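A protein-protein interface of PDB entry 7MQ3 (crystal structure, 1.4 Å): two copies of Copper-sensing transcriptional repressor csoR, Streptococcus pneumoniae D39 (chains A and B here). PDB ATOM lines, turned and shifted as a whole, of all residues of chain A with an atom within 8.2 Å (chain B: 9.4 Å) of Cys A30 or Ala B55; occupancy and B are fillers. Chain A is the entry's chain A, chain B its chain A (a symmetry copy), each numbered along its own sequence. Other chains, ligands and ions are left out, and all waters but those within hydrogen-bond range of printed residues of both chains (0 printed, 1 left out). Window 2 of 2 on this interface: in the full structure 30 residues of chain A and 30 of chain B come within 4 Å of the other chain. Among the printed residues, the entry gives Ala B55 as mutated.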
ATOM      1  N   MET A  23     -39.033  -0.397  -9.910  1.00  0.00           N
ATOM      2  CA  MET A  23     -38.032  -1.305  -9.362  1.00  0.00           C
ATOM      3  C   MET A  23     -37.610  -0.869  -7.966  1.00  0.00           C
ATOM      4  O   MET A  23     -37.415  -1.706  -7.076  1.00  0.00           O
ATOM      5  CB  MET A  23     -36.821  -1.359 -10.292  1.00  0.00           C
ATOM      6  CG  MET A  23     -37.129  -1.908 -11.675  1.00  0.00           C
ATOM      7  SD  MET A  23     -35.721  -1.766 -12.792  1.00  0.00           S
ATOM      8  CE  MET A  23     -34.701  -3.123 -12.220  1.00  0.00           C
ATOM      9  N   ILE A  24     -37.476   0.441  -7.752  1.00  0.00           N
ATOM     10  CA  ILE A  24     -37.104   0.941  -6.433  1.00  0.00           C
ATOM     11  C   ILE A  24     -38.255   0.773  -5.453  1.00  0.00           C
ATOM     12  O   ILE A  24     -38.057   0.350  -4.307  1.00  0.00           O
ATOM     13  CB  ILE A  24     -36.641   2.406  -6.529  1.00  0.00           C
ATOM     14  CG1 ILE A  24     -35.327   2.490  -7.306  1.00  0.00           C
ATOM     15  CG2 ILE A  24     -36.490   2.998  -5.140  1.00  0.00           C
ATOM     16  CD1 ILE A  24     -35.035   3.867  -7.862  1.00  0.00           C
ATOM     17  N   ASP A  27     -38.028  -2.669  -4.183  1.00  0.00           N
ATOM     18  CA  ASP A  27     -36.775  -3.109  -3.578  1.00  0.00           C
ATOM     19  C   ASP A  27     -36.084  -4.162  -4.439  1.00  0.00           C
ATOM     20  O   ASP A  27     -35.494  -5.123  -3.938  1.00  0.00           O
ATOM     21  CB  ASP A  27     -36.994  -3.604  -2.148  1.00  0.00           C
ATOM     22  CG  ASP A  27     -37.368  -2.482  -1.198  1.00  0.00           C
ATOM     23  OD1 ASP A  27     -36.565  -1.536  -1.049  1.00  0.00           O
ATOM     24  OD2 ASP A  27     -38.466  -2.543  -0.603  1.00  0.00           O
ATOM     25  N   ARG A  28     -36.149  -3.970  -5.754  1.00  0.00           N
ATOM     26  CA  ARG A  28     -35.453  -4.850  -6.677  1.00  0.00           C
ATOM     27  C   ARG A  28     -33.945  -4.779  -6.445  1.00  0.00           C
ATOM     28  O   ARG A  28     -33.426  -3.852  -5.816  1.00  0.00           O
ATOM     29  CB  ARG A  28     -35.763  -4.446  -8.117  1.00  0.00           C
ATOM     30  CG  ARG A  28     -37.169  -4.788  -8.568  1.00  0.00           C
ATOM     31  CD  ARG A  28     -37.280  -6.265  -8.911  1.00  0.00           C
ATOM     32  NE  ARG A  28     -36.374  -6.647  -9.994  1.00  0.00           N
ATOM     33  CZ  ARG A  28     -36.619  -6.445 -11.283  1.00  0.00           C
ATOM     34  NH1 ARG A  28     -37.749  -5.865 -11.666  1.00  0.00           N
ATOM     35  NH2 ARG A  28     -35.734  -6.828 -12.194  1.00  0.00           N
ATOM     36  N   ASP A  29     -33.241  -5.781  -6.966  1.00  0.00           N
ATOM     37  CA  ASP A  29     -31.807  -5.880  -6.742  1.00  0.00           C
ATOM     38  C   ASP A  29     -31.116  -4.624  -7.250  1.00  0.00           C
ATOM     39  O   ASP A  29     -31.369  -4.171  -8.371  1.00  0.00           O
ATOM     40  CB  ASP A  29     -31.250  -7.114  -7.455  1.00  0.00           C
ATOM     41  CG  ASP A  29     -31.363  -8.376  -6.615  1.00  0.00           C
ATOM     42  OD1 ASP A  29     -31.487  -8.265  -5.375  1.00  0.00           O
ATOM     43  OD2 ASP A  29     -31.335  -9.483  -7.192  1.00  0.00           O
ATOM     44  N   CYS A  30     -30.249  -4.053  -6.411  1.00  0.00           N
ATOM     45  CA  CYS A  30     -29.518  -2.850  -6.788  1.00  0.00           C
ATOM     46  C   CYS A  30     -28.853  -3.009  -8.150  1.00  0.00           C
ATOM     47  O   CYS A  30     -28.796  -2.057  -8.934  1.00  0.00           O
ATOM     48  CB  CYS A  30     -28.480  -2.528  -5.711  1.00  0.00           C
ATOM     49  SG  CYS A  30     -27.062  -1.554  -6.249  1.00  0.00           S
ATOM     50  N   ALA A  31     -28.357  -4.209  -8.451  1.00  0.00           N
ATOM     51  CA  ALA A  31     -27.626  -4.408  -9.698  1.00  0.00           C
ATOM     52  C   ALA A  31     -28.537  -4.236 -10.906  1.00  0.00           C
ATOM     53  O   ALA A  31     -28.139  -3.628 -11.908  1.00  0.00           O
ATOM     54  CB  ALA A  31     -26.975  -5.791  -9.705  1.00  0.00           C
ATOM     55  N   ASP A  32     -29.762  -4.760 -10.834  1.00  0.00           N
ATOM     56  CA  ASP A  32     -30.723  -4.549 -11.911  1.00  0.00           C
ATOM     57  C   ASP A  32     -31.063  -3.070 -12.056  1.00  0.00           C
ATOM     58  O   ASP A  32     -31.111  -2.535 -13.170  1.00  0.00           O
ATOM     59  CB  ASP A  32     -31.992  -5.360 -11.644  1.00  0.00           C
ATOM     60  CG  ASP A  32     -31.763  -6.857 -11.740  1.00  0.00           C
ATOM     61  OD1 ASP A  32     -31.006  -7.292 -12.632  1.00  0.00           O
ATOM     62  OD2 ASP A  32     -32.345  -7.598 -10.922  1.00  0.00           O
ATOM     63  N   ILE A  33     -31.309  -2.393 -10.933  1.00  0.00           N
ATOM     64  CA  ILE A  33     -31.636  -0.971 -10.978  1.00  0.00           C
ATOM     65  C   ILE A  33     -30.486  -0.180 -11.584  1.00  0.00           C
ATOM     66  O   ILE A  33     -30.695   0.703 -12.425  1.00  0.00           O
ATOM     67  CB  ILE A  33     -32.005  -0.466  -9.572  1.00  0.00           C
ATOM     68  CG1 ILE A  33     -33.341  -1.065  -9.130  1.00  0.00           C
ATOM     69  CG2 ILE A  33     -32.068   1.049  -9.547  1.00  0.00           C
ATOM     70  CD1 ILE A  33     -33.612  -0.932  -7.652  1.00  0.00           C
ATOM     71  N   VAL A  34     -29.254  -0.485 -11.171  1.00  0.00           N
ATOM     72  CA  VAL A  34     -28.093   0.230 -11.685  1.00  0.00           C
ATOM     73  C   VAL A  34     -27.910  -0.035 -13.173  1.00  0.00           C
ATOM     74  O   VAL A  34     -27.615   0.881 -13.950  1.00  0.00           O
ATOM     75  CB  VAL A  34     -26.838  -0.140 -10.872  1.00  0.00           C
ATOM     76  CG1 VAL A  34     -25.584   0.299 -11.603  1.00  0.00           C
ATOM     77  CG2 VAL A  34     -26.906   0.478  -9.475  1.00  0.00           C
ATOM     78  N   THR A  35     -28.084  -1.287 -13.599  1.00  0.00           N
ATOM     79  CA  THR A  35     -27.997  -1.602 -15.021  1.00  0.00           C
ATOM     80  C   THR A  35     -28.975  -0.755 -15.825  1.00  0.00           C
ATOM     81  O   THR A  35     -28.614  -0.178 -16.858  1.00  0.00           O
ATOM     82  CB  THR A  35     -28.273  -3.092 -15.233  1.00  0.00           C
ATOM     83  OG1 THR A  35     -27.191  -3.867 -14.698  1.00  0.00           O
ATOM     84  CG2 THR A  35     -28.431  -3.402 -16.717  1.00  0.00           C
ATOM     85  N   GLN A  36     -30.222  -0.663 -15.361  1.00  0.00           N
ATOM     86  CA  GLN A  36     -31.227   0.093 -16.098  1.00  0.00           C
ATOM     87  C   GLN A  36     -30.937   1.587 -16.050  1.00  0.00           C
ATOM     88  O   GLN A  36     -31.063   2.284 -17.064  1.00  0.00           O
ATOM     89  CB  GLN A  36     -32.617  -0.203 -15.538  1.00  0.00           C
ATOM     90  CG  GLN A  36     -33.021  -1.663 -15.632  1.00  0.00           C
ATOM     91  CD  GLN A  36     -34.193  -1.886 -16.567  1.00  0.00           C
ATOM     92  OE1 GLN A  36     -35.280  -1.344 -16.360  1.00  0.00           O
ATOM     93  NE2 GLN A  36     -33.978  -2.686 -17.605  1.00  0.00           N
ATOM     94  N   LEU A  37     -30.542   2.101 -14.885  1.00  0.00           N
ATOM     95  CA  LEU A  37     -30.180   3.511 -14.804  1.00  0.00           C
ATOM     96  C   LEU A  37     -28.998   3.829 -15.711  1.00  0.00           C
ATOM     97  O   LEU A  37     -28.947   4.904 -16.318  1.00  0.00           O
ATOM     98  CB  LEU A  37     -29.861   3.890 -13.360  1.00  0.00           C
ATOM     99  CG  LEU A  37     -31.067   4.095 -12.447  1.00  0.00           C
ATOM    100  CD1 LEU A  37     -30.606   4.202 -10.998  1.00  0.00           C
ATOM    101  CD2 LEU A  37     -31.851   5.325 -12.853  1.00  0.00           C
ATOM    102  N   TYR B   6     -35.095   8.236  -3.966  1.00  0.00           N
ATOM    103  CA  TYR B   6     -34.596   7.976  -5.310  1.00  0.00           C
ATOM    104  C   TYR B   6     -35.721   7.906  -6.329  1.00  0.00           C
ATOM    105  O   TYR B   6     -35.526   8.297  -7.485  1.00  0.00           O
ATOM    106  CB  TYR B   6     -33.783   6.684  -5.324  1.00  0.00           C
ATOM    107  CG  TYR B   6     -32.613   6.730  -4.378  1.00  0.00           C
ATOM    108  CD1 TYR B   6     -31.744   7.813  -4.375  1.00  0.00           C
ATOM    109  CD2 TYR B   6     -32.383   5.701  -3.477  1.00  0.00           C
ATOM    110  CE1 TYR B   6     -30.676   7.868  -3.506  1.00  0.00           C
ATOM    111  CE2 TYR B   6     -31.316   5.746  -2.605  1.00  0.00           C
ATOM    112  CZ  TYR B   6     -30.466   6.832  -2.625  1.00  0.00           C
ATOM    113  OH  TYR B   6     -29.401   6.890  -1.761  1.00  0.00           O
ATOM    114  N   VAL B  47     -27.938   9.377  -8.757  1.00  0.00           N
ATOM    115  CA  VAL B  47     -28.786   8.328  -8.200  1.00  0.00           C
ATOM    116  C   VAL B  47     -28.061   6.988  -8.226  1.00  0.00           C
ATOM    117  O   VAL B  47     -28.104   6.225  -7.256  1.00  0.00           O
ATOM    118  CB  VAL B  47     -30.132   8.264  -8.945  1.00  0.00           C
ATOM    119  CG1 VAL B  47     -30.891   7.008  -8.535  1.00  0.00           C
ATOM    120  CG2 VAL B  47     -30.952   9.508  -8.662  1.00  0.00           C
ATOM    121  N   ILE B  48     -27.390   6.682  -9.339  1.00  0.00           N
ATOM    122  CA  ILE B  48     -26.594   5.459  -9.410  1.00  0.00           C
ATOM    123  C   ILE B  48     -25.613   5.401  -8.248  1.00  0.00           C
ATOM    124  O   ILE B  48     -25.521   4.398  -7.533  1.00  0.00           O
ATOM    125  CB  ILE B  48     -25.871   5.364 -10.765  1.00  0.00           C
ATOM    126  CG1 ILE B  48     -26.875   5.141 -11.897  1.00  0.00           C
ATOM    127  CG2 ILE B  48     -24.843   4.239 -10.734  1.00  0.00           C
ATOM    128  CD1 ILE B  48     -26.284   5.321 -13.281  1.00  0.00           C
ATOM    129  N   GLU B  49     -24.862   6.485  -8.044  1.00  0.00           N
ATOM    130  CA  GLU B  49     -23.845   6.491  -7.001  1.00  0.00           C
ATOM    131  C   GLU B  49     -24.466   6.306  -5.622  1.00  0.00           C
ATOM    132  O   GLU B  49     -23.958   5.532  -4.803  1.00  0.00           O
ATOM    133  CB  GLU B  49     -23.052   7.797  -7.060  1.00  0.00           C
ATOM    134  CG  GLU B  49     -22.045   7.860  -8.194  1.00  0.00           C
ATOM    135  CD  GLU B  49     -21.351   9.205  -8.281  1.00  0.00           C
ATOM    136  OE1 GLU B  49     -21.421   9.977  -7.302  1.00  0.00           O
ATOM    137  OE2 GLU B  49     -20.734   9.489  -9.329  1.00  0.00           O
ATOM    138  N   MET B  50     -25.569   7.005  -5.346  1.00  0.00           N
ATOM    139  CA  MET B  50     -26.180   6.909  -4.026  1.00  0.00           C
ATOM    140  C   MET B  50     -26.800   5.539  -3.794  1.00  0.00           C
ATOM    141  O   MET B  50     -26.763   5.025  -2.670  1.00  0.00           O
ATOM    142  CB  MET B  50     -27.220   8.014  -3.853  1.00  0.00           C
ATOM    143  CG  MET B  50     -26.626   9.415  -3.884  1.00  0.00           C
ATOM    144  SD  MET B  50     -27.861  10.716  -4.047  1.00  0.00           S
ATOM    145  CE  MET B  50     -28.614  10.676  -2.423  1.00  0.00           C
ATOM    146  N   ILE B  51     -27.355   4.922  -4.839  1.00  0.00           N
ATOM    147  CA  ILE B  51     -27.939   3.594  -4.683  1.00  0.00           C
ATOM    148  C   ILE B  51     -26.856   2.558  -4.414  1.00  0.00           C
ATOM    149  O   ILE B  51     -27.014   1.683  -3.554  1.00  0.00           O
ATOM    150  CB  ILE B  51     -28.797   3.231  -5.909  1.00  0.00           C
ATOM    151  CG1 ILE B  51     -30.117   4.001  -5.863  1.00  0.00           C
ATOM    152  CG2 ILE B  51     -29.060   1.738  -5.958  1.00  0.00           C
ATOM    153  CD1 ILE B  51     -30.990   3.810  -7.076  1.00  0.00           C
ATOM    154  N   ILE B  52     -25.739   2.634  -5.141  1.00  0.00           N
ATOM    155  CA  ILE B  52     -24.630   1.722  -4.875  1.00  0.00           C
ATOM    156  C   ILE B  52     -24.099   1.935  -3.466  1.00  0.00           C
ATOM    157  O   ILE B  52     -23.844   0.973  -2.731  1.00  0.00           O
ATOM    158  CB  ILE B  52     -23.528   1.885  -5.938  1.00  0.00           C
ATOM    159  CG1 ILE B  52     -24.030   1.388  -7.294  1.00  0.00           C
ATOM    160  CG2 ILE B  52     -22.273   1.130  -5.522  1.00  0.00           C
ATOM    161  CD1 ILE B  52     -23.207   1.877  -8.467  1.00  0.00           C
ATOM    162  N   THR B  53     -23.924   3.194  -3.064  1.00  0.00           N
ATOM    163  CA  THR B  53     -23.401   3.479  -1.732  1.00  0.00           C
ATOM    164  C   THR B  53     -24.328   2.928  -0.659  1.00  0.00           C
ATOM    165  O   THR B  53     -23.877   2.302   0.306  1.00  0.00           O
ATOM    166  CB  THR B  53     -23.214   4.986  -1.557  1.00  0.00           C
ATOM    167  OG1 THR B  53     -22.200   5.449  -2.456  1.00  0.00           O
ATOM    168  CG2 THR B  53     -22.806   5.318  -0.127  1.00  0.00           C
ATOM    169  N   GLU B  54     -25.635   3.145  -0.815  1.00  0.00           N
ATOM    170  CA  GLU B  54     -26.586   2.586   0.139  1.00  0.00           C
ATOM    171  C   GLU B  54     -26.493   1.067   0.184  1.00  0.00           C
ATOM    172  O   GLU B  54     -26.490   0.471   1.265  1.00  0.00           O
ATOM    173  CB  GLU B  54     -28.006   3.020  -0.216  1.00  0.00           C
ATOM    174  CG  GLU B  54     -28.387   4.387   0.318  1.00  0.00           C
ATOM    175  CD  GLU B  54     -29.887   4.599   0.369  1.00  0.00           C
ATOM    176  OE1 GLU B  54     -30.640   3.612   0.227  1.00  0.00           O
ATOM    177  OE2 GLU B  54     -30.314   5.757   0.554  1.00  0.00           O
ATOM    178  N   ALA B  55     -26.413   0.422  -0.983  1.00  0.00           N
ATOM    179  CA  ALA B  55     -26.368  -1.036  -1.015  1.00  0.00           C
ATOM    180  C   ALA B  55     -25.135  -1.561  -0.295  1.00  0.00           C
ATOM    181  O   ALA B  55     -25.217  -2.526   0.473  1.00  0.00           O
ATOM    182  CB  ALA B  55     -26.391  -1.530  -2.460  1.00  0.00           C
ATOM    183  N   LEU B  56     -23.979  -0.938  -0.525  1.00  0.00           N
ATOM    184  CA  LEU B  56     -22.756  -1.407   0.114  1.00  0.00           C
ATOM    185  C   LEU B  56     -22.766  -1.118   1.611  1.00  0.00           C
ATOM    186  O   LEU B  56     -22.293  -1.932   2.409  1.00  0.00           O
ATOM    187  CB  LEU B  56     -21.542  -0.746  -0.538  1.00  0.00           C
ATOM    188  CG  LEU B  56     -21.294  -1.076  -2.007  1.00  0.00           C
ATOM    189  CD1 LEU B  56     -20.020  -0.420  -2.511  1.00  0.00           C
ATOM    190  CD2 LEU B  56     -21.234  -2.582  -2.200  1.00  0.00           C
ATOM    191  N   THR B  57     -23.292   0.043   2.007  1.00  0.00           N
ATOM    192  CA  THR B  57     -23.378   0.354   3.430  1.00  0.00           C
ATOM    193  C   THR B  57     -24.291  -0.630   4.147  1.00  0.00           C
ATOM    194  O   THR B  57     -24.004  -1.049   5.275  1.00  0.00           O
ATOM    195  CB  THR B  57     -23.873   1.787   3.620  1.00  0.00           C
ATOM    196  OG1 THR B  57     -22.942   2.695   3.022  1.00  0.00           O
ATOM    197  CG2 THR B  57     -24.009   2.112   5.098  1.00  0.00           C
ATOM    198  N   GLU B  58     -25.396  -1.011   3.507  1.00  0.00           N
ATOM    199  CA  GLU B  58     -26.275  -2.022   4.081  1.00  0.00           C
ATOM    200  C   GLU B  58     -25.572  -3.368   4.180  1.00  0.00           C
ATOM    201  O   GLU B  58     -25.698  -4.079   5.188  1.00  0.00           O
ATOM    202  CB  GLU B  58     -27.564  -2.135   3.261  1.00  0.00           C
ATOM    203  CG  GLU B  58     -28.646  -2.955   4.043  1.00  0.00           C
ATOM    204  CD  GLU B  58     -29.991  -2.928   3.287  1.00  0.00           C
ATOM    205  OE1 GLU B  58     -30.084  -3.609   2.251  1.00  0.00           O
ATOM    206  OE2 GLU B  58     -30.833  -2.114   3.613  1.00  0.00           O
ATOM    207  N   CYS B  59     -24.844  -3.758   3.131  1.00  0.00           N
ATOM    208  CA  CYS B  59     -24.032  -4.966   3.205  1.00  0.00           C
ATOM    209  C   CYS B  59     -23.133  -4.931   4.431  1.00  0.00           C
ATOM    210  O   CYS B  59     -23.100  -5.880   5.224  1.00  0.00           O
ATOM    211  CB  CYS B  59     -23.192  -5.101   1.935  1.00  0.00           C
ATOM    212  SG  CYS B  59     -24.111  -5.692   0.502  1.00  0.00           S
ATOM    213  N   ILE B  60     -22.404  -3.828   4.608  1.00  0.00           N
ATOM    214  CA  ILE B  60     -21.428  -3.742   5.687  1.00  0.00           C
ATOM    215  C   ILE B  60     -22.121  -3.819   7.040  1.00  0.00           C
ATOM    216  O   ILE B  60     -21.639  -4.486   7.963  1.00  0.00           O
ATOM    217  CB  ILE B  60     -20.600  -2.450   5.545  1.00  0.00           C
ATOM    218  CG1 ILE B  60     -19.721  -2.518   4.293  1.00  0.00           C
ATOM    219  CG2 ILE B  60     -19.760  -2.227   6.793  1.00  0.00           C
ATOM    220  CD1 ILE B  60     -19.190  -1.178   3.840  1.00  0.00           C
ATOM    221  N   ASN B  61     -23.253  -3.138   7.179  1.00  0.00           N
ATOM    222  CA  ASN B  61     -23.877  -2.933   8.478  1.00  0.00           C
ATOM    223  C   ASN B  61     -24.950  -3.966   8.787  1.00  0.00           C
ATOM    224  O   ASN B  61     -25.476  -3.975   9.907  1.00  0.00           O
ATOM    225  CB  ASN B  61     -24.472  -1.525   8.546  1.00  0.00           C
ATOM    226  CG  ASN B  61     -23.406  -0.456   8.662  1.00  0.00           C
ATOM    227  OD1 ASN B  61     -23.150   0.292   7.717  1.00  0.00           O
ATOM    228  ND2 ASN B  61     -22.771  -0.384   9.820  1.00  0.00           N
ATOM    229  N   GLN B  62     -25.270  -4.844   7.841  1.00  0.00           N
ATOM    230  CA  GLN B  62     -26.140  -5.992   8.077  1.00  0.00           C
ATOM    231  C   GLN B  62     -25.397  -7.277   7.709  1.00  0.00           C
ATOM    232  O   GLN B  62     -25.797  -7.998   6.793  1.00  0.00           O
ATOM    233  CB  GLN B  62     -27.430  -5.871   7.270  1.00  0.00           C
ATOM    234  CG  GLN B  62     -28.221  -4.607   7.542  1.00  0.00           C
ATOM    235  CD  GLN B  62     -29.519  -4.557   6.758  1.00  0.00           C
ATOM    236  OE1 GLN B  62     -29.674  -5.242   5.745  1.00  0.00           O
ATOM    237  NE2 GLN B  62     -30.460  -3.742   7.222  1.00  0.00           N
ATOM    238  N   GLN B  70     -19.321 -13.302   4.858  1.00  0.00           N
ATOM    239  CA  GLN B  70     -19.533 -11.862   4.786  1.00  0.00           C
ATOM    240  C   GLN B  70     -18.421 -11.185   3.997  1.00  0.00           C
ATOM    241  O   GLN B  70     -18.682 -10.287   3.192  1.00  0.00           O
ATOM    242  CB  GLN B  70     -19.626 -11.279   6.193  1.00  0.00           C
ATOM    243  CG  GLN B  70     -19.732  -9.767   6.249  1.00  0.00           C
ATOM    244  CD  GLN B  70     -20.999  -9.229   5.621  1.00  0.00           C
ATOM    245  OE1 GLN B  70     -21.937  -9.967   5.325  1.00  0.00           O
ATOM    246  NE2 GLN B  70     -21.030  -7.922   5.416  1.00  0.00           N
ATOM    247  N   ARG B  73     -19.123 -11.754   0.418  1.00  0.00           N
ATOM    248  CA  ARG B  73     -20.224 -10.872   0.051  1.00  0.00           C
ATOM    249  C   ARG B  73     -19.739  -9.448  -0.167  1.00  0.00           C
ATOM    250  O   ARG B  73     -20.089  -8.808  -1.165  1.00  0.00           O
ATOM    251  CB  ARG B  73     -21.278 -10.926   1.152  1.00  0.00           C
ATOM    252  CG  ARG B  73     -22.542 -10.163   0.879  1.00  0.00           C
ATOM    253  CD  ARG B  73     -23.326 -10.071   2.174  1.00  0.00           C
ATOM    254  NE  ARG B  73     -24.492  -9.207   2.072  1.00  0.00           N
ATOM    255  CZ  ARG B  73     -25.137  -8.712   3.121  1.00  0.00           C
ATOM    256  NH1 ARG B  73     -24.721  -8.995   4.350  1.00  0.00           N
ATOM    257  NH2 ARG B  73     -26.197  -7.941   2.946  1.00  0.00           N
ATOM    258  N   LEU B  74     -18.928  -8.924   0.754  1.00  0.00           N
ATOM    259  CA  LEU B  74     -18.423  -7.567   0.583  1.00  0.00           C
ATOM    260  C   LEU B  74     -17.535  -7.466  -0.651  1.00  0.00           C
ATOM    261  O   LEU B  74     -17.583  -6.471  -1.382  1.00  0.00           O
ATOM    262  CB  LEU B  74     -17.650  -7.134   1.826  1.00  0.00           C
ATOM    263  CG  LEU B  74     -18.460  -6.826   3.085  1.00  0.00           C
ATOM    264  CD1 LEU B  74     -17.513  -6.676   4.281  1.00  0.00           C
ATOM    265  CD2 LEU B  74     -19.301  -5.585   2.912  1.00  0.00           C
ATOM    266  N   ALA B  77     -19.370  -7.164  -3.689  1.00  0.00           N
ATOM    267  CA  ALA B  77     -20.055  -5.880  -3.743  1.00  0.00           C
ATOM    268  C   ALA B  77     -19.104  -4.745  -4.094  1.00  0.00           C
ATOM    269  O   ALA B  77     -19.502  -3.797  -4.782  1.00  0.00           O
ATOM    270  CB  ALA B  77     -20.750  -5.604  -2.407  1.00  0.00           C
ATOM    271  N   ILE B  78     -17.854  -4.815  -3.643  1.00  0.00           N
ATOM    272  CA  ILE B  78     -16.929  -3.719  -3.908  1.00  0.00           C
ATOM    273  C   ILE B  78     -16.451  -3.740  -5.353  1.00  0.00           C
ATOM    274  O   ILE B  78     -16.410  -2.699  -6.016  1.00  0.00           O
ATOM    275  CB  ILE B  78     -15.758  -3.742  -2.908  1.00  0.00           C
ATOM    276  CG1 ILE B  78     -15.021  -5.082  -2.959  1.00  0.00           C
ATOM    277  CG2 ILE B  78     -16.257  -3.445  -1.497  1.00  0.00           C
ATOM    278  CD1 ILE B  78     -13.502  -4.928  -2.994  1.00  0.00           C
ATOM    279  N   TYR B  80     -18.051  -4.747  -7.774  1.00  0.00           N
ATOM    280  CA  TYR B  80     -19.158  -4.126  -8.493  1.00  0.00           C
ATOM    281  C   TYR B  80     -19.079  -2.607  -8.434  1.00  0.00           C
ATOM    282  O   TYR B  80     -19.293  -1.929  -9.446  1.00  0.00           O
ATOM    283  CB  TYR B  80     -20.472  -4.616  -7.897  1.00  0.00           C
ATOM    284  CG  TYR B  80     -21.678  -4.130  -8.640  1.00  0.00           C
ATOM    285  CD1 TYR B  80     -22.082  -4.743  -9.814  1.00  0.00           C
ATOM    286  CD2 TYR B  80     -22.409  -3.048  -8.175  1.00  0.00           C
ATOM    287  CE1 TYR B  80     -23.186  -4.301 -10.502  1.00  0.00           C
ATOM    288  CE2 TYR B  80     -23.514  -2.597  -8.856  1.00  0.00           C
ATOM    289  CZ  TYR B  80     -23.897  -3.226 -10.020  1.00  0.00           C
ATOM    290  OH  TYR B  80     -24.996  -2.779 -10.703  1.00  0.00           O
ATOM    291  N   LEU B  81     -18.785  -2.048  -7.258  1.00  0.00           N
ATOM    292  CA  LEU B  81     -18.631  -0.603  -7.143  1.00  0.00           C
ATOM    293  C   LEU B  81     -17.560  -0.095  -8.099  1.00  0.00           C
ATOM    294  O   LEU B  81     -17.802   0.817  -8.897  1.00  0.00           O
ATOM    295  CB  LEU B  81     -18.287  -0.235  -5.702  1.00  0.00           C
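Ile A24 touches Tyr B6 (CD1 to CB, 3.99 Å). Ile B51 touches Cys A30 (CG2 to SG, 3.9 Å). SG of Cys A30 touches CB of Ala B55, 3.8 Å away. CD1 of Ile B51 touches CG2 of Ile A33, at 3.9 Å. CG2 of Val A34 touches CG1 of Ile B52, at 3.7 Å. Val A34 touches Tyr B80 (CB to OH, 3.2 Å). Val B47 touches Leu A37. Ile B48 touches Leu A37 (CG1 to CB, 3.6 Å). Ile B51 touches Leu A37.
The backbone carbonyl oxygen (O) of Ala A31 lies close to the side-chain hydroxyl (OH) of Tyr B80 (3.5 Å).
The side-chain hydroxyl of Thr A35 lies within hydrogen-bond range of the backbone carbonyl oxygen of Ala A31, at 3.0 Å. OH of Tyr B6 sits close to O of Met B50 (3.4 Å). The side-chain carboxylate of Glu B54 is in hydrogen-bond range of the side-chain hydroxyl of Tyr B6 (2.7 Å). The backbone carbonyl oxygen (O) of Ala B55 is in hydrogen-bond range of the side-chain sulfur (SG) of Cys B59 (3.4 Å).
Of the 13 printed residues of chain A, 6 touch a printed residue of chain B. Printed residues of chain A that touch a printed residue of chain B: Ile A24, Cys A30, Ala A31, Ile A33, Val A34 and Leu A37. Hydrophobic or aromatic side chains of chain A that line the printed part of chain B: Ile A24, Ala A31, Ile A33, Val A34 and Leu A37. Of the 24 printed residues of chain B, 7 touch a printed residue of chain A. Printed residues of chain B that touch a printed residue of chain A: Tyr B6, Val B47, Ile B48, Ile B51, Ile B52, Ala B55 and Tyr B80. Along chain B the printed residues that touch a printed residue of chain A span positions 6 to 80. Among the printed residues, no Asp or Glu carboxylate lies within 4 Å of a Lys or Arg side-chain nitrogen of the other chain.
No position is printed for both chains. Of the 10 pairs that touch across the chains among the printed residues, none has its exchanged pair printed and touching as well.
Ala A31 touches just one residue of chain B: Tyr B80 (3.3 Å). Ile A33 touches just one residue of chain B: Ile B51 (3.9 Å). Of the printed residues of chain B, Leu A37 touches Val B47 (3.7 Å), Ile B48 (3.6 Å) and Ile B51 (3.96 Å). Printed residues of chain A within 4 Å of Val B47: Leu A37. Of the printed residues of chain A, Ile B51 touches Cys A30 (3.9 Å), Ile A33 (3.9 Å) and Leu A37 (3.96 Å). Printed residues of chain A within 4 Å of Ile B52: Val A34 (3.7 Å). Asn B61 touches none of the printed residues of chain A. The nearest residue of chain A that does not touch Ala B55 is Ala A31 (6.9 Å).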
